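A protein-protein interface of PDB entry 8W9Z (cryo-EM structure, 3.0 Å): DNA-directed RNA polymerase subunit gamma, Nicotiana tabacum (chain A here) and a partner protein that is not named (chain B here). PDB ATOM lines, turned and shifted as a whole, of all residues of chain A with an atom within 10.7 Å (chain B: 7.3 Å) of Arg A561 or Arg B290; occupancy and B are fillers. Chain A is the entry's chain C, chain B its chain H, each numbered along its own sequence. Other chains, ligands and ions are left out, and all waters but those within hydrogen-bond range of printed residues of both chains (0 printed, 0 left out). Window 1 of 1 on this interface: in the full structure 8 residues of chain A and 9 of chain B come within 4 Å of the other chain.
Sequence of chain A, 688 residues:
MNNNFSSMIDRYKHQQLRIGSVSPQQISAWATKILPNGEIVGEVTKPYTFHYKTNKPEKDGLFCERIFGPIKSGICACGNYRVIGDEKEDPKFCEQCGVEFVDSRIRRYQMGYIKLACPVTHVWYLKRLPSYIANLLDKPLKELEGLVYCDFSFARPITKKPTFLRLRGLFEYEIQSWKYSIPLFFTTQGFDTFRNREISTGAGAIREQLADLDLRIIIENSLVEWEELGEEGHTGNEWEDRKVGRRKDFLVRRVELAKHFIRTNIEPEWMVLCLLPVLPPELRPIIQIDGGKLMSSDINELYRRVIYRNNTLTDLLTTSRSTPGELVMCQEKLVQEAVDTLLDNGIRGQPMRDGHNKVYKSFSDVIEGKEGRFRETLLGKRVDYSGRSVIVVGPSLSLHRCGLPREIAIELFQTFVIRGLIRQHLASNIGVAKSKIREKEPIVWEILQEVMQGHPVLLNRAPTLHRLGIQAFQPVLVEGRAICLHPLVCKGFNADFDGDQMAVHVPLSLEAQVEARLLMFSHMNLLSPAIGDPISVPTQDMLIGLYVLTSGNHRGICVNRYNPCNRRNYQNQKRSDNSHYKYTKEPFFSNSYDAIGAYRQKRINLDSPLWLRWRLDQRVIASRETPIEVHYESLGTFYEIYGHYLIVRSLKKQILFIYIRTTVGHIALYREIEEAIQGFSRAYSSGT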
ATOM      1  N   HIS A 554      -2.447   6.162 -36.314  1.00  0.00           N
ATOM      2  CA  HIS A 554      -1.773   7.345 -35.803  1.00  0.00           C
ATOM      3  C   HIS A 554      -0.437   7.542 -36.511  1.00  0.00           C
ATOM      4  O   HIS A 554       0.167   6.596 -37.023  1.00  0.00           O
ATOM      5  CB  HIS A 554      -1.560   7.216 -34.296  1.00  0.00           C
ATOM      6  CG  HIS A 554      -2.770   6.737 -33.555  1.00  0.00           C
ATOM      7  ND1 HIS A 554      -3.095   5.402 -33.447  1.00  0.00           N
ATOM      8  CD2 HIS A 554      -3.737   7.415 -32.894  1.00  0.00           C
ATOM      9  CE1 HIS A 554      -4.209   5.278 -32.746  1.00  0.00           C
ATOM     10  NE2 HIS A 554      -4.618   6.484 -32.399  1.00  0.00           N
ATOM     11  N   ARG A 555       0.026   8.791 -36.536  1.00  0.00           N
ATOM     12  CA  ARG A 555       1.238   9.142 -37.265  1.00  0.00           C
ATOM     13  C   ARG A 555       2.255   9.940 -36.461  1.00  0.00           C
ATOM     14  O   ARG A 555       3.437   9.923 -36.824  1.00  0.00           O
ATOM     15  CB  ARG A 555       0.889   9.940 -38.531  1.00  0.00           C
ATOM     16  CG  ARG A 555      -0.050   9.220 -39.485  1.00  0.00           C
ATOM     17  CD  ARG A 555      -0.398  10.093 -40.680  1.00  0.00           C
ATOM     18  NE  ARG A 555      -1.360   9.447 -41.568  1.00  0.00           N
ATOM     19  CZ  ARG A 555      -2.678   9.562 -41.449  1.00  0.00           C
ATOM     20  NH1 ARG A 555      -3.480   8.940 -42.303  1.00  0.00           N
ATOM     21  NH2 ARG A 555      -3.198  10.297 -40.476  1.00  0.00           N
ATOM     22  N   GLY A 556       1.854  10.629 -35.397  1.00  0.00           N
ATOM     23  CA  GLY A 556       2.774  11.497 -34.688  1.00  0.00           C
ATOM     24  C   GLY A 556       3.050  11.096 -33.254  1.00  0.00           C
ATOM     25  O   GLY A 556       3.640  10.043 -32.998  1.00  0.00           O
ATOM     26  N   ILE A 557       2.629  11.938 -32.307  1.00  0.00           N
ATOM     27  CA  ILE A 557       2.883  11.671 -30.897  1.00  0.00           C
ATOM     28  C   ILE A 557       2.117  10.454 -30.399  1.00  0.00           C
ATOM     29  O   ILE A 557       2.438   9.919 -29.332  1.00  0.00           O
ATOM     30  CB  ILE A 557       2.531  12.903 -30.044  1.00  0.00           C
ATOM     31  CG1 ILE A 557       1.065  13.287 -30.243  1.00  0.00           C
ATOM     32  CG2 ILE A 557       3.443  14.069 -30.388  1.00  0.00           C
ATOM     33  CD1 ILE A 557       0.621  14.449 -29.390  1.00  0.00           C
ATOM     34  N   CYS A 558       1.108  10.000 -31.143  1.00  0.00           N
ATOM     35  CA  CYS A 558       0.300   8.870 -30.705  1.00  0.00           C
ATOM     36  C   CYS A 558       0.916   7.526 -31.068  1.00  0.00           C
ATOM     37  O   CYS A 558       0.455   6.496 -30.564  1.00  0.00           O
ATOM     38  CB  CYS A 558      -1.105   8.974 -31.298  1.00  0.00           C
ATOM     39  SG  CYS A 558      -1.971  10.512 -30.915  1.00  0.00           S
ATOM     40  N   VAL A 559       1.938   7.506 -31.924  1.00  0.00           N
ATOM     41  CA  VAL A 559       2.606   6.269 -32.288  1.00  0.00           C
ATOM     42  C   VAL A 559       4.010   6.168 -31.698  1.00  0.00           C
ATOM     43  O   VAL A 559       4.483   5.055 -31.444  1.00  0.00           O
ATOM     44  CB  VAL A 559       2.642   6.096 -33.824  1.00  0.00           C
ATOM     45  CG1 VAL A 559       3.543   7.139 -34.468  1.00  0.00           C
ATOM     46  CG2 VAL A 559       3.075   4.686 -34.202  1.00  0.00           C
ATOM     47  N   ASN A 560       4.682   7.291 -31.455  1.00  0.00           N
ATOM     48  CA  ASN A 560       5.987   7.314 -30.811  1.00  0.00           C
ATOM     49  C   ASN A 560       5.908   8.146 -29.540  1.00  0.00           C
ATOM     50  O   ASN A 560       5.252   9.192 -29.513  1.00  0.00           O
ATOM     51  CB  ASN A 560       7.064   7.888 -31.739  1.00  0.00           C
ATOM     52  CG  ASN A 560       7.502   6.905 -32.804  1.00  0.00           C
ATOM     53  OD1 ASN A 560       8.412   6.105 -32.589  1.00  0.00           O
ATOM     54  ND2 ASN A 560       6.860   6.964 -33.964  1.00  0.00           N
ATOM     55  N   ARG A 561       6.581   7.680 -28.488  1.00  0.00           N
ATOM     56  CA  ARG A 561       6.553   8.401 -27.220  1.00  0.00           C
ATOM     57  C   ARG A 561       7.538   9.564 -27.222  1.00  0.00           C
ATOM     58  O   ARG A 561       7.161  10.712 -26.966  1.00  0.00           O
ATOM     59  CB  ARG A 561       6.852   7.449 -26.059  1.00  0.00           C
ATOM     60  CG  ARG A 561       6.779   8.123 -24.700  1.00  0.00           C
ATOM     61  CD  ARG A 561       7.148   7.177 -23.573  1.00  0.00           C
ATOM     62  NE  ARG A 561       7.097   7.844 -22.276  1.00  0.00           N
ATOM     63  CZ  ARG A 561       7.391   7.255 -21.122  1.00  0.00           C
ATOM     64  NH1 ARG A 561       7.317   7.940 -19.989  1.00  0.00           N
ATOM     65  NH2 ARG A 561       7.759   5.982 -21.099  1.00  0.00           N
ATOM     66  N   TYR A 562       8.803   9.283 -27.508  1.00  0.00           N
ATOM     67  CA  TYR A 562       9.844  10.296 -27.530  1.00  0.00           C
ATOM     68  C   TYR A 562      10.124  10.744 -28.961  1.00  0.00           C
ATOM     69  O   TYR A 562       9.690  10.124 -29.933  1.00  0.00           O
ATOM     70  CB  TYR A 562      11.121   9.766 -26.872  1.00  0.00           C
ATOM     71  CG  TYR A 562      10.961   9.452 -25.402  1.00  0.00           C
ATOM     72  CD1 TYR A 562      10.063  10.158 -24.615  1.00  0.00           C
ATOM     73  CD2 TYR A 562      11.706   8.448 -24.802  1.00  0.00           C
ATOM     74  CE1 TYR A 562       9.913   9.876 -23.273  1.00  0.00           C
ATOM     75  CE2 TYR A 562      11.563   8.158 -23.460  1.00  0.00           C
ATOM     76  CZ  TYR A 562      10.665   8.874 -22.701  1.00  0.00           C
ATOM     77  OH  TYR A 562      10.519   8.589 -21.363  1.00  0.00           O
ATOM     78  N   ASN A 563      10.857  11.844 -29.076  1.00  0.00           N
ATOM     79  CA  ASN A 563      11.154  12.413 -30.384  1.00  0.00           C
ATOM     80  C   ASN A 563      12.066  11.473 -31.164  1.00  0.00           C
ATOM     81  O   ASN A 563      13.119  11.073 -30.654  1.00  0.00           O
ATOM     82  CB  ASN A 563      11.808  13.784 -30.226  1.00  0.00           C
ATOM     83  CG  ASN A 563      11.768  14.606 -31.500  1.00  0.00           C
ATOM     84  OD1 ASN A 563      11.981  14.090 -32.596  1.00  0.00           O
ATOM     85  ND2 ASN A 563      11.494  15.896 -31.360  1.00  0.00           N
ATOM     86  N   PRO A 564      11.702  11.096 -32.394  1.00  0.00           N
ATOM     87  CA  PRO A 564      12.552  10.188 -33.180  1.00  0.00           C
ATOM     88  C   PRO A 564      13.885  10.785 -33.605  1.00  0.00           C
ATOM     89  O   PRO A 564      14.629  10.125 -34.338  1.00  0.00           O
ATOM     90  CB  PRO A 564      11.682   9.870 -34.406  1.00  0.00           C
ATOM     91  CG  PRO A 564      10.287  10.192 -33.986  1.00  0.00           C
ATOM     92  CD  PRO A 564      10.411  11.351 -33.054  1.00  0.00           C
ATOM     93  N   CYS A 565      14.212  12.008 -33.183  1.00  0.00           N
ATOM     94  CA  CYS A 565      15.476  12.630 -33.559  1.00  0.00           C
ATOM     95  C   CYS A 565      16.683  11.951 -32.925  1.00  0.00           C
ATOM     96  O   CYS A 565      17.817  12.261 -33.307  1.00  0.00           O
ATOM     97  CB  CYS A 565      15.454  14.113 -33.178  1.00  0.00           C
ATOM     98  SG  CYS A 565      16.758  15.116 -33.933  1.00  0.00           S
ATOM     99  N   ASN A 566      16.475  11.034 -31.979  1.00  0.00           N
ATOM    100  CA  ASN A 566      17.578  10.373 -31.295  1.00  0.00           C
ATOM    101  C   ASN A 566      17.943   9.022 -31.896  1.00  0.00           C
ATOM    102  O   ASN A 566      19.097   8.600 -31.768  1.00  0.00           O
ATOM    103  CB  ASN A 566      17.243  10.181 -29.810  1.00  0.00           C
ATOM    104  CG  ASN A 566      16.895  11.485 -29.121  1.00  0.00           C
ATOM    105  OD1 ASN A 566      15.790  11.649 -28.603  1.00  0.00           O
ATOM    106  ND2 ASN A 566      17.838  12.419 -29.110  1.00  0.00           N
ATOM    107  N   LEU B 212      13.420  16.278 -26.330  1.00  0.00           N
ATOM    108  CA  LEU B 212      13.360  14.820 -26.319  1.00  0.00           C
ATOM    109  C   LEU B 212      11.930  14.317 -26.157  1.00  0.00           C
ATOM    110  O   LEU B 212      11.557  13.300 -26.752  1.00  0.00           O
ATOM    111  CB  LEU B 212      14.246  14.263 -25.206  1.00  0.00           C
ATOM    112  CG  LEU B 212      15.738  14.586 -25.290  1.00  0.00           C
ATOM    113  CD1 LEU B 212      16.505  13.848 -24.205  1.00  0.00           C
ATOM    114  CD2 LEU B 212      16.287  14.250 -26.666  1.00  0.00           C
ATOM    115  N   GLY B 213      11.120  15.009 -25.363  1.00  0.00           N
ATOM    116  CA  GLY B 213       9.760  14.594 -25.095  1.00  0.00           C
ATOM    117  C   GLY B 213       9.515  14.036 -23.711  1.00  0.00           C
ATOM    118  O   GLY B 213       8.463  13.427 -23.487  1.00  0.00           O
ATOM    119  N   ARG B 214      10.446  14.221 -22.779  1.00  0.00           N
ATOM    120  CA  ARG B 214      10.290  13.703 -21.434  1.00  0.00           C
ATOM    121  C   ARG B 214       9.248  14.520 -20.671  1.00  0.00           C
ATOM    122  O   ARG B 214       8.892  15.627 -21.084  1.00  0.00           O
ATOM    123  CB  ARG B 214      11.633  13.729 -20.710  1.00  0.00           C
ATOM    124  CG  ARG B 214      12.755  13.057 -21.484  1.00  0.00           C
ATOM    125  CD  ARG B 214      14.047  13.030 -20.688  1.00  0.00           C
ATOM    126  NE  ARG B 214      13.979  12.096 -19.569  1.00  0.00           N
ATOM    127  CZ  ARG B 214      14.346  10.820 -19.640  1.00  0.00           C
ATOM    128  NH1 ARG B 214      14.807  10.323 -20.779  1.00  0.00           N
ATOM    129  NH2 ARG B 214      14.251  10.041 -18.571  1.00  0.00           N
ATOM    130  N   PRO B 215       8.724  13.985 -19.565  1.00  0.00           N
ATOM    131  CA  PRO B 215       7.745  14.743 -18.768  1.00  0.00           C
ATOM    132  C   PRO B 215       8.300  16.087 -18.322  1.00  0.00           C
ATOM    133  O   PRO B 215       9.345  16.166 -17.672  1.00  0.00           O
ATOM    134  CB  PRO B 215       7.472  13.817 -17.579  1.00  0.00           C
ATOM    135  CG  PRO B 215       7.723  12.457 -18.111  1.00  0.00           C
ATOM    136  CD  PRO B 215       8.858  12.597 -19.087  1.00  0.00           C
ATOM    137  N   LEU B 263      -3.797   7.208 -14.669  1.00  0.00           N
ATOM    138  CA  LEU B 263      -2.756   8.214 -14.501  1.00  0.00           C
ATOM    139  C   LEU B 263      -2.147   8.146 -13.108  1.00  0.00           C
ATOM    140  O   LEU B 263      -0.927   8.253 -12.956  1.00  0.00           O
ATOM    141  CB  LEU B 263      -3.314   9.608 -14.774  1.00  0.00           C
ATOM    142  CG  LEU B 263      -3.436  10.001 -16.245  1.00  0.00           C
ATOM    143  CD1 LEU B 263      -3.968  11.415 -16.381  1.00  0.00           C
ATOM    144  CD2 LEU B 263      -2.096   9.863 -16.937  1.00  0.00           C
ATOM    145  N   MET B 266       0.087   4.950 -12.943  1.00  0.00           N
ATOM    146  CA  MET B 266       1.365   5.080 -13.632  1.00  0.00           C
ATOM    147  C   MET B 266       2.229   6.205 -13.079  1.00  0.00           C
ATOM    148  O   MET B 266       3.445   6.198 -13.305  1.00  0.00           O
ATOM    149  CB  MET B 266       1.151   5.284 -15.135  1.00  0.00           C
ATOM    150  CG  MET B 266       0.433   6.561 -15.512  1.00  0.00           C
ATOM    151  SD  MET B 266       0.305   6.731 -17.300  1.00  0.00           S
ATOM    152  CE  MET B 266      -0.300   5.106 -17.737  1.00  0.00           C
ATOM    153  N   GLY B 270       6.689   5.407 -10.837  1.00  0.00           N
ATOM    154  CA  GLY B 270       7.611   6.249 -11.575  1.00  0.00           C
ATOM    155  C   GLY B 270       7.649   6.050 -13.074  1.00  0.00           C
ATOM    156  O   GLY B 270       8.738   6.026 -13.661  1.00  0.00           O
ATOM    157  N   GLN B 271       6.492   5.909 -13.718  1.00  0.00           N
ATOM    158  CA  GLN B 271       6.476   5.832 -15.174  1.00  0.00           C
ATOM    159  C   GLN B 271       6.272   7.197 -15.818  1.00  0.00           C
ATOM    160  O   GLN B 271       6.954   7.528 -16.795  1.00  0.00           O
ATOM    161  CB  GLN B 271       5.391   4.865 -15.649  1.00  0.00           C
ATOM    162  CG  GLN B 271       5.433   4.599 -17.145  1.00  0.00           C
ATOM    163  CD  GLN B 271       4.471   3.513 -17.579  1.00  0.00           C
ATOM    164  OE1 GLN B 271       4.487   3.080 -18.730  1.00  0.00           O
ATOM    165  NE2 GLN B 271       3.628   3.065 -16.657  1.00  0.00           N
ATOM    166  N   VAL B 272       5.346   7.999 -15.294  1.00  0.00           N
ATOM    167  CA  VAL B 272       5.123   9.361 -15.754  1.00  0.00           C
ATOM    168  C   VAL B 272       5.199  10.293 -14.552  1.00  0.00           C
ATOM    169  O   VAL B 272       5.157   9.865 -13.399  1.00  0.00           O
ATOM    170  CB  VAL B 272       3.772   9.529 -16.482  1.00  0.00           C
ATOM    171  CG1 VAL B 272       3.637   8.515 -17.607  1.00  0.00           C
ATOM    172  CG2 VAL B 272       2.623   9.410 -15.499  1.00  0.00           C
ATOM    173  N   LYS B 273       5.317  11.586 -14.839  1.00  0.00           N
ATOM    174  CA  LYS B 273       5.367  12.623 -13.818  1.00  0.00           C
ATOM    175  C   LYS B 273       4.245  13.620 -14.068  1.00  0.00           C
ATOM    176  O   LYS B 273       4.096  14.123 -15.186  1.00  0.00           O
ATOM    177  CB  LYS B 273       6.722  13.335 -13.815  1.00  0.00           C
ATOM    178  CG  LYS B 273       7.894  12.436 -13.460  1.00  0.00           C
ATOM    179  CD  LYS B 273       9.198  13.213 -13.437  1.00  0.00           C
ATOM    180  CE  LYS B 273      10.372  12.312 -13.094  1.00  0.00           C
ATOM    181  NZ  LYS B 273      10.211  11.672 -11.760  1.00  0.00           N
ATOM    182  N   THR B 284      -5.620  14.250 -18.448  1.00  0.00           N
ATOM    183  CA  THR B 284      -6.483  13.146 -18.855  1.00  0.00           C
ATOM    184  C   THR B 284      -6.764  13.191 -20.353  1.00  0.00           C
ATOM    185  O   THR B 284      -6.776  12.150 -21.021  1.00  0.00           O
ATOM    186  CB  THR B 284      -7.789  13.176 -18.064  1.00  0.00           C
ATOM    187  OG1 THR B 284      -8.437  14.440 -18.251  1.00  0.00           O
ATOM    188  CG2 THR B 284      -7.523  12.960 -16.584  1.00  0.00           C
ATOM    189  N   ALA B 285      -6.984  14.388 -20.900  1.00  0.00           N
ATOM    190  CA  ALA B 285      -7.217  14.514 -22.334  1.00  0.00           C
ATOM    191  C   ALA B 285      -5.984  14.113 -23.134  1.00  0.00           C
ATOM    192  O   ALA B 285      -6.102  13.539 -24.222  1.00  0.00           O
ATOM    193  CB  ALA B 285      -7.638  15.942 -22.675  1.00  0.00           C
ATOM    194  N   LEU B 286      -4.793  14.409 -22.612  1.00  0.00           N
ATOM    195  CA  LEU B 286      -3.566  14.000 -23.289  1.00  0.00           C
ATOM    196  C   LEU B 286      -3.354  12.494 -23.185  1.00  0.00           C
ATOM    197  O   LEU B 286      -2.908  11.858 -24.147  1.00  0.00           O
ATOM    198  CB  LEU B 286      -2.374  14.754 -22.706  1.00  0.00           C
ATOM    199  CG  LEU B 286      -0.988  14.401 -23.246  1.00  0.00           C
ATOM    200  CD1 LEU B 286      -0.893  14.705 -24.730  1.00  0.00           C
ATOM    201  CD2 LEU B 286       0.086  15.148 -22.476  1.00  0.00           C
ATOM    202  N   TYR B 287      -3.664  11.910 -22.027  1.00  0.00           N
ATOM    203  CA  TYR B 287      -3.553  10.465 -21.864  1.00  0.00           C
ATOM    204  C   TYR B 287      -4.541   9.722 -22.753  1.00  0.00           C
ATOM    205  O   TYR B 287      -4.257   8.601 -23.189  1.00  0.00           O
ATOM    206  CB  TYR B 287      -3.769  10.087 -20.398  1.00  0.00           C
ATOM    207  CG  TYR B 287      -3.898   8.603 -20.150  1.00  0.00           C
ATOM    208  CD1 TYR B 287      -2.775   7.794 -20.066  1.00  0.00           C
ATOM    209  CD2 TYR B 287      -5.143   8.012 -19.988  1.00  0.00           C
ATOM    210  CE1 TYR B 287      -2.889   6.439 -19.837  1.00  0.00           C
ATOM    211  CE2 TYR B 287      -5.266   6.658 -19.760  1.00  0.00           C
ATOM    212  CZ  TYR B 287      -4.135   5.876 -19.684  1.00  0.00           C
ATOM    213  OH  TYR B 287      -4.253   4.526 -19.456  1.00  0.00           O
ATOM    214  N   ARG B 288      -5.701  10.324 -23.023  1.00  0.00           N
ATOM    215  CA  ARG B 288      -6.672   9.691 -23.908  1.00  0.00           C
ATOM    216  C   ARG B 288      -6.106   9.490 -25.308  1.00  0.00           C
ATOM    217  O   ARG B 288      -6.501   8.551 -26.009  1.00  0.00           O
ATOM    218  CB  ARG B 288      -7.948  10.529 -23.962  1.00  0.00           C
ATOM    219  CG  ARG B 288      -9.137   9.826 -24.587  1.00  0.00           C
ATOM    220  CD  ARG B 288     -10.328  10.761 -24.665  1.00  0.00           C
ATOM    221  NE  ARG B 288     -10.626  11.364 -23.371  1.00  0.00           N
ATOM    222  CZ  ARG B 288     -11.543  12.307 -23.181  1.00  0.00           C
ATOM    223  NH1 ARG B 288     -12.257  12.756 -24.204  1.00  0.00           N
ATOM    224  NH2 ARG B 288     -11.747  12.799 -21.968  1.00  0.00           N
ATOM    225  N   ALA B 289      -5.183  10.354 -25.732  1.00  0.00           N
ATOM    226  CA  ALA B 289      -4.542  10.219 -27.032  1.00  0.00           C
ATOM    227  C   ALA B 289      -3.337   9.289 -26.990  1.00  0.00           C
ATOM    228  O   ALA B 289      -3.162   8.460 -27.890  1.00  0.00           O
ATOM    229  CB  ALA B 289      -4.118  11.594 -27.556  1.00  0.00           C
ATOM    230  N   ARG B 290      -2.503   9.410 -25.962  1.00  0.00           N
ATOM    231  CA  ARG B 290      -1.320   8.569 -25.792  1.00  0.00           C
ATOM    232  C   ARG B 290      -1.639   7.540 -24.715  1.00  0.00           C
ATOM    233  O   ARG B 290      -1.355   7.738 -23.534  1.00  0.00           O
ATOM    234  CB  ARG B 290      -0.108   9.413 -25.425  1.00  0.00           C
ATOM    235  CG  ARG B 290      -0.010  10.710 -26.200  1.00  0.00           C
ATOM    236  CD  ARG B 290       1.151  11.542 -25.705  1.00  0.00           C
ATOM    237  NE  ARG B 290       2.434  10.911 -25.992  1.00  0.00           N
ATOM    238  CZ  ARG B 290       3.587  11.304 -25.466  1.00  0.00           C
ATOM    239  NH1 ARG B 290       4.711  10.680 -25.783  1.00  0.00           N
ATOM    240  NH2 ARG B 290       3.615  12.320 -24.616  1.00  0.00           N
ATOM    241  N   ARG B 291      -2.241   6.433 -25.130  1.00  0.00           N
ATOM    242  CA  ARG B 291      -2.655   5.378 -24.215  1.00  0.00           C
ATOM    243  C   ARG B 291      -2.045   4.028 -24.550  1.00  0.00           C
ATOM    244  O   ARG B 291      -1.709   3.265 -23.641  1.00  0.00           O
ATOM    245  CB  ARG B 291      -4.186   5.258 -24.212  1.00  0.00           C
ATOM    246  CG  ARG B 291      -4.735   4.289 -23.181  1.00  0.00           C
ATOM    247  CD  ARG B 291      -6.139   3.811 -23.538  1.00  0.00           C
ATOM    248  NE  ARG B 291      -7.084   4.911 -23.705  1.00  0.00           N
ATOM    249  CZ  ARG B 291      -7.509   5.360 -24.882  1.00  0.00           C
ATOM    250  NH1 ARG B 291      -7.073   4.803 -26.003  1.00  0.00           N
ATOM    251  NH2 ARG B 291      -8.370   6.366 -24.938  1.00  0.00           N
ATOM    252  N   HIS B 292      -1.890   3.714 -25.837  1.00  0.00           N
ATOM    253  CA  HIS B 292      -1.368   2.418 -26.246  1.00  0.00           C
ATOM    254  C   HIS B 292       0.142   2.312 -26.085  1.00  0.00           C
ATOM    255  O   HIS B 292       0.660   1.196 -25.962  1.00  0.00           O
ATOM    256  CB  HIS B 292      -1.752   2.139 -27.698  1.00  0.00           C
ATOM    257  CG  HIS B 292      -3.218   2.271 -27.970  1.00  0.00           C
ATOM    258  ND1 HIS B 292      -3.846   3.493 -28.082  1.00  0.00           N
ATOM    259  CD2 HIS B 292      -4.181   1.336 -28.146  1.00  0.00           C
ATOM    260  CE1 HIS B 292      -5.132   3.304 -28.318  1.00  0.00           C
ATOM    261  NE2 HIS B 292      -5.361   2.003 -28.362  1.00  0.00           N
ATOM    262  N   LEU B 293       0.853   3.441 -26.082  1.00  0.00           N
ATOM    263  CA  LEU B 293       2.305   3.408 -25.939  1.00  0.00           C
ATOM    264  C   LEU B 293       2.709   2.802 -24.601  1.00  0.00           C
ATOM    265  O   LEU B 293       3.573   1.918 -24.538  1.00  0.00           O
ATOM    266  CB  LEU B 293       2.871   4.820 -26.084  1.00  0.00           C
ATOM    267  CG  LEU B 293       2.336   5.644 -27.255  1.00  0.00           C
ATOM    268  CD1 LEU B 293       2.903   7.050 -27.225  1.00  0.00           C
ATOM    269  CD2 LEU B 293       2.654   4.965 -28.576  1.00  0.00           C
ATOM    270  N   TYR B 294       2.084   3.263 -23.518  1.00  0.00           N
ATOM    271  CA  TYR B 294       2.424   2.757 -22.195  1.00  0.00           C
ATOM    272  C   TYR B 294       1.991   1.308 -22.018  1.00  0.00           C
ATOM    273  O   TYR B 294       2.681   0.535 -21.343  1.00  0.00           O
ATOM    274  CB  TYR B 294       1.795   3.648 -21.126  1.00  0.00           C
ATOM    275  CG  TYR B 294       2.081   5.118 -21.332  1.00  0.00           C
ATOM    276  CD1 TYR B 294       3.252   5.690 -20.857  1.00  0.00           C
ATOM    277  CD2 TYR B 294       1.183   5.932 -22.006  1.00  0.00           C
ATOM    278  CE1 TYR B 294       3.519   7.032 -21.046  1.00  0.00           C
ATOM    279  CE2 TYR B 294       1.442   7.274 -22.201  1.00  0.00           C
ATOM    280  CZ  TYR B 294       2.610   7.818 -21.717  1.00  0.00           C
ATOM    281  OH  TYR B 294       2.871   9.154 -21.908  1.00  0.00           O
ATOM    282  N   LYS B 295       0.865   0.920 -22.621  1.00  0.00           N
ATOM    283  CA  LYS B 295       0.456  -0.480 -22.580  1.00  0.00           C
ATOM    284  C   LYS B 295       1.472  -1.368 -23.285  1.00  0.00           C
ATOM    285  O   LYS B 295       1.831  -2.439 -22.780  1.00  0.00           O
ATOM    286  CB  LYS B 295      -0.927  -0.643 -23.208  1.00  0.00           C
ATOM    287  CG  LYS B 295      -1.449  -2.068 -23.198  1.00  0.00           C
ATOM    288  CD  LYS B 295      -2.811  -2.163 -23.865  1.00  0.00           C
ATOM    289  CE  LYS B 295      -3.833  -1.286 -23.162  1.00  0.00           C
ATOM    290  NZ  LYS B 295      -5.171  -1.361 -23.812  1.00  0.00           N
ATOM    291  N   GLU B 297       4.627  -0.669 -23.686  1.00  0.00           N
ATOM    292  CA  GLU B 297       5.826  -0.681 -22.853  1.00  0.00           C
ATOM    293  C   GLU B 297       5.689  -1.668 -21.699  1.00  0.00           C
ATOM    294  O   GLU B 297       6.629  -2.412 -21.392  1.00  0.00           O
ATOM    295  CB  GLU B 297       6.118   0.722 -22.326  1.00  0.00           C
ATOM    296  CG  GLU B 297       6.578   1.699 -23.394  1.00  0.00           C
ATOM    297  CD  GLU B 297       6.927   3.060 -22.828  1.00  0.00           C
ATOM    298  OE1 GLU B 297       6.783   3.250 -21.602  1.00  0.00           O
ATOM    299  OE2 GLU B 297       7.348   3.939 -23.609  1.00  0.00           O
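The backbone NH of Asn A563 is in hydrogen-bond range of the backbone carbonyl oxygen of Leu B212, 2.8 Å away. NH2 of Arg A561 is in salt-bridge range of OE1 of Glu B297, 2.9 Å away. O of Arg A561 is in hydrogen-bond range of NH1 of Arg B290, 2.7 Å away. The guanidinium group of Arg B290 sits at hydrogen-bond distance from the backbone carbonyl oxygen of Ile A557 (3.5 Å). NH1 of Arg A561 is in hydrogen-bond range of O of Gln B271 (3.2 Å).
Of the printed residues of chain B, Cys A558 touches Ala B289 (3.8 Å) and Leu B293 (3.3 Å). Printed residues of chain B within 4 Å of Arg A561: Gln B271 (3.2 Å), Arg B290 (2.7 Å), Leu B293 (3.9 Å), Tyr B294 (3.9 Å) and Glu B297 (2.9 Å). Of the printed residues of chain B, Tyr A562 touches Leu B212 and Gly B213. Gly B213 touches just one residue of chain A: Tyr A562. Gly B270 touches none of the printed residues of chain A. No residue of chain A comes within 4 Å of Leu B286. No residue of chain A comes within 4 Å of Tyr B287. Of chain A, only Cys A558 comes within 4 Å of Ala B289. Arg B290 touches two residues of chain A. The nearest residue of chain A that does not touch Arg B290 is Asn A560 (4.1 Å).
OD1 of Asn A566 lies close to O of Asn A563 (3.4 Å). O of Met B266 lies within hydrogen-bond range of N of Gln B271 (3.1 Å). OD1 of Asn A563 sits close to N of Cys A565, 3.1 Å away.
CD1 of Leu B293 touches O of Ile A557 (3.6 Å). SG of Cys A558 touches O of Ala B289, at 3.8 Å. Cys A558 touches Leu B293 (O to CD2, 3.3 Å). Val A559 touches Leu B293 (O to CD2, 3.4 Å). Asn A560 touches Leu B293. Arg A561 touches Leu B293. Arg A561 touches Tyr B294 (NE to CE1, 3.9 Å). Tyr A562 touches Leu B212. CD1 of Tyr A562 touches O of Gly B213, 3.8 Å away. Asn A566 touches Leu B212.
Of the 23 printed residues of chain B, 8 touch a printed residue of chain A. Printed residues of chain B that touch a printed residue of chain A: Leu B212, Gly B213, Gln B271, Ala B289, Arg B290, Leu B293, Tyr B294 and Glu B297. Hydrophobic or aromatic side chains of chain B that line the printed part of chain A: Leu B212, Leu B293 and Tyr B294. Along chain B the printed residues that touch a printed residue of chain A span positions 212 to 297. Of the 13 printed residues of chain A, 8 touch a printed residue of chain B. Among the printed residues, 15 pairs touch across the chains. Among the printed residues, Asp or Glu carboxylates within 4 Å of a Lys or Arg side-chain nitrogen of the other chain: Arg A561 with Glu B297 (2.9 Å).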
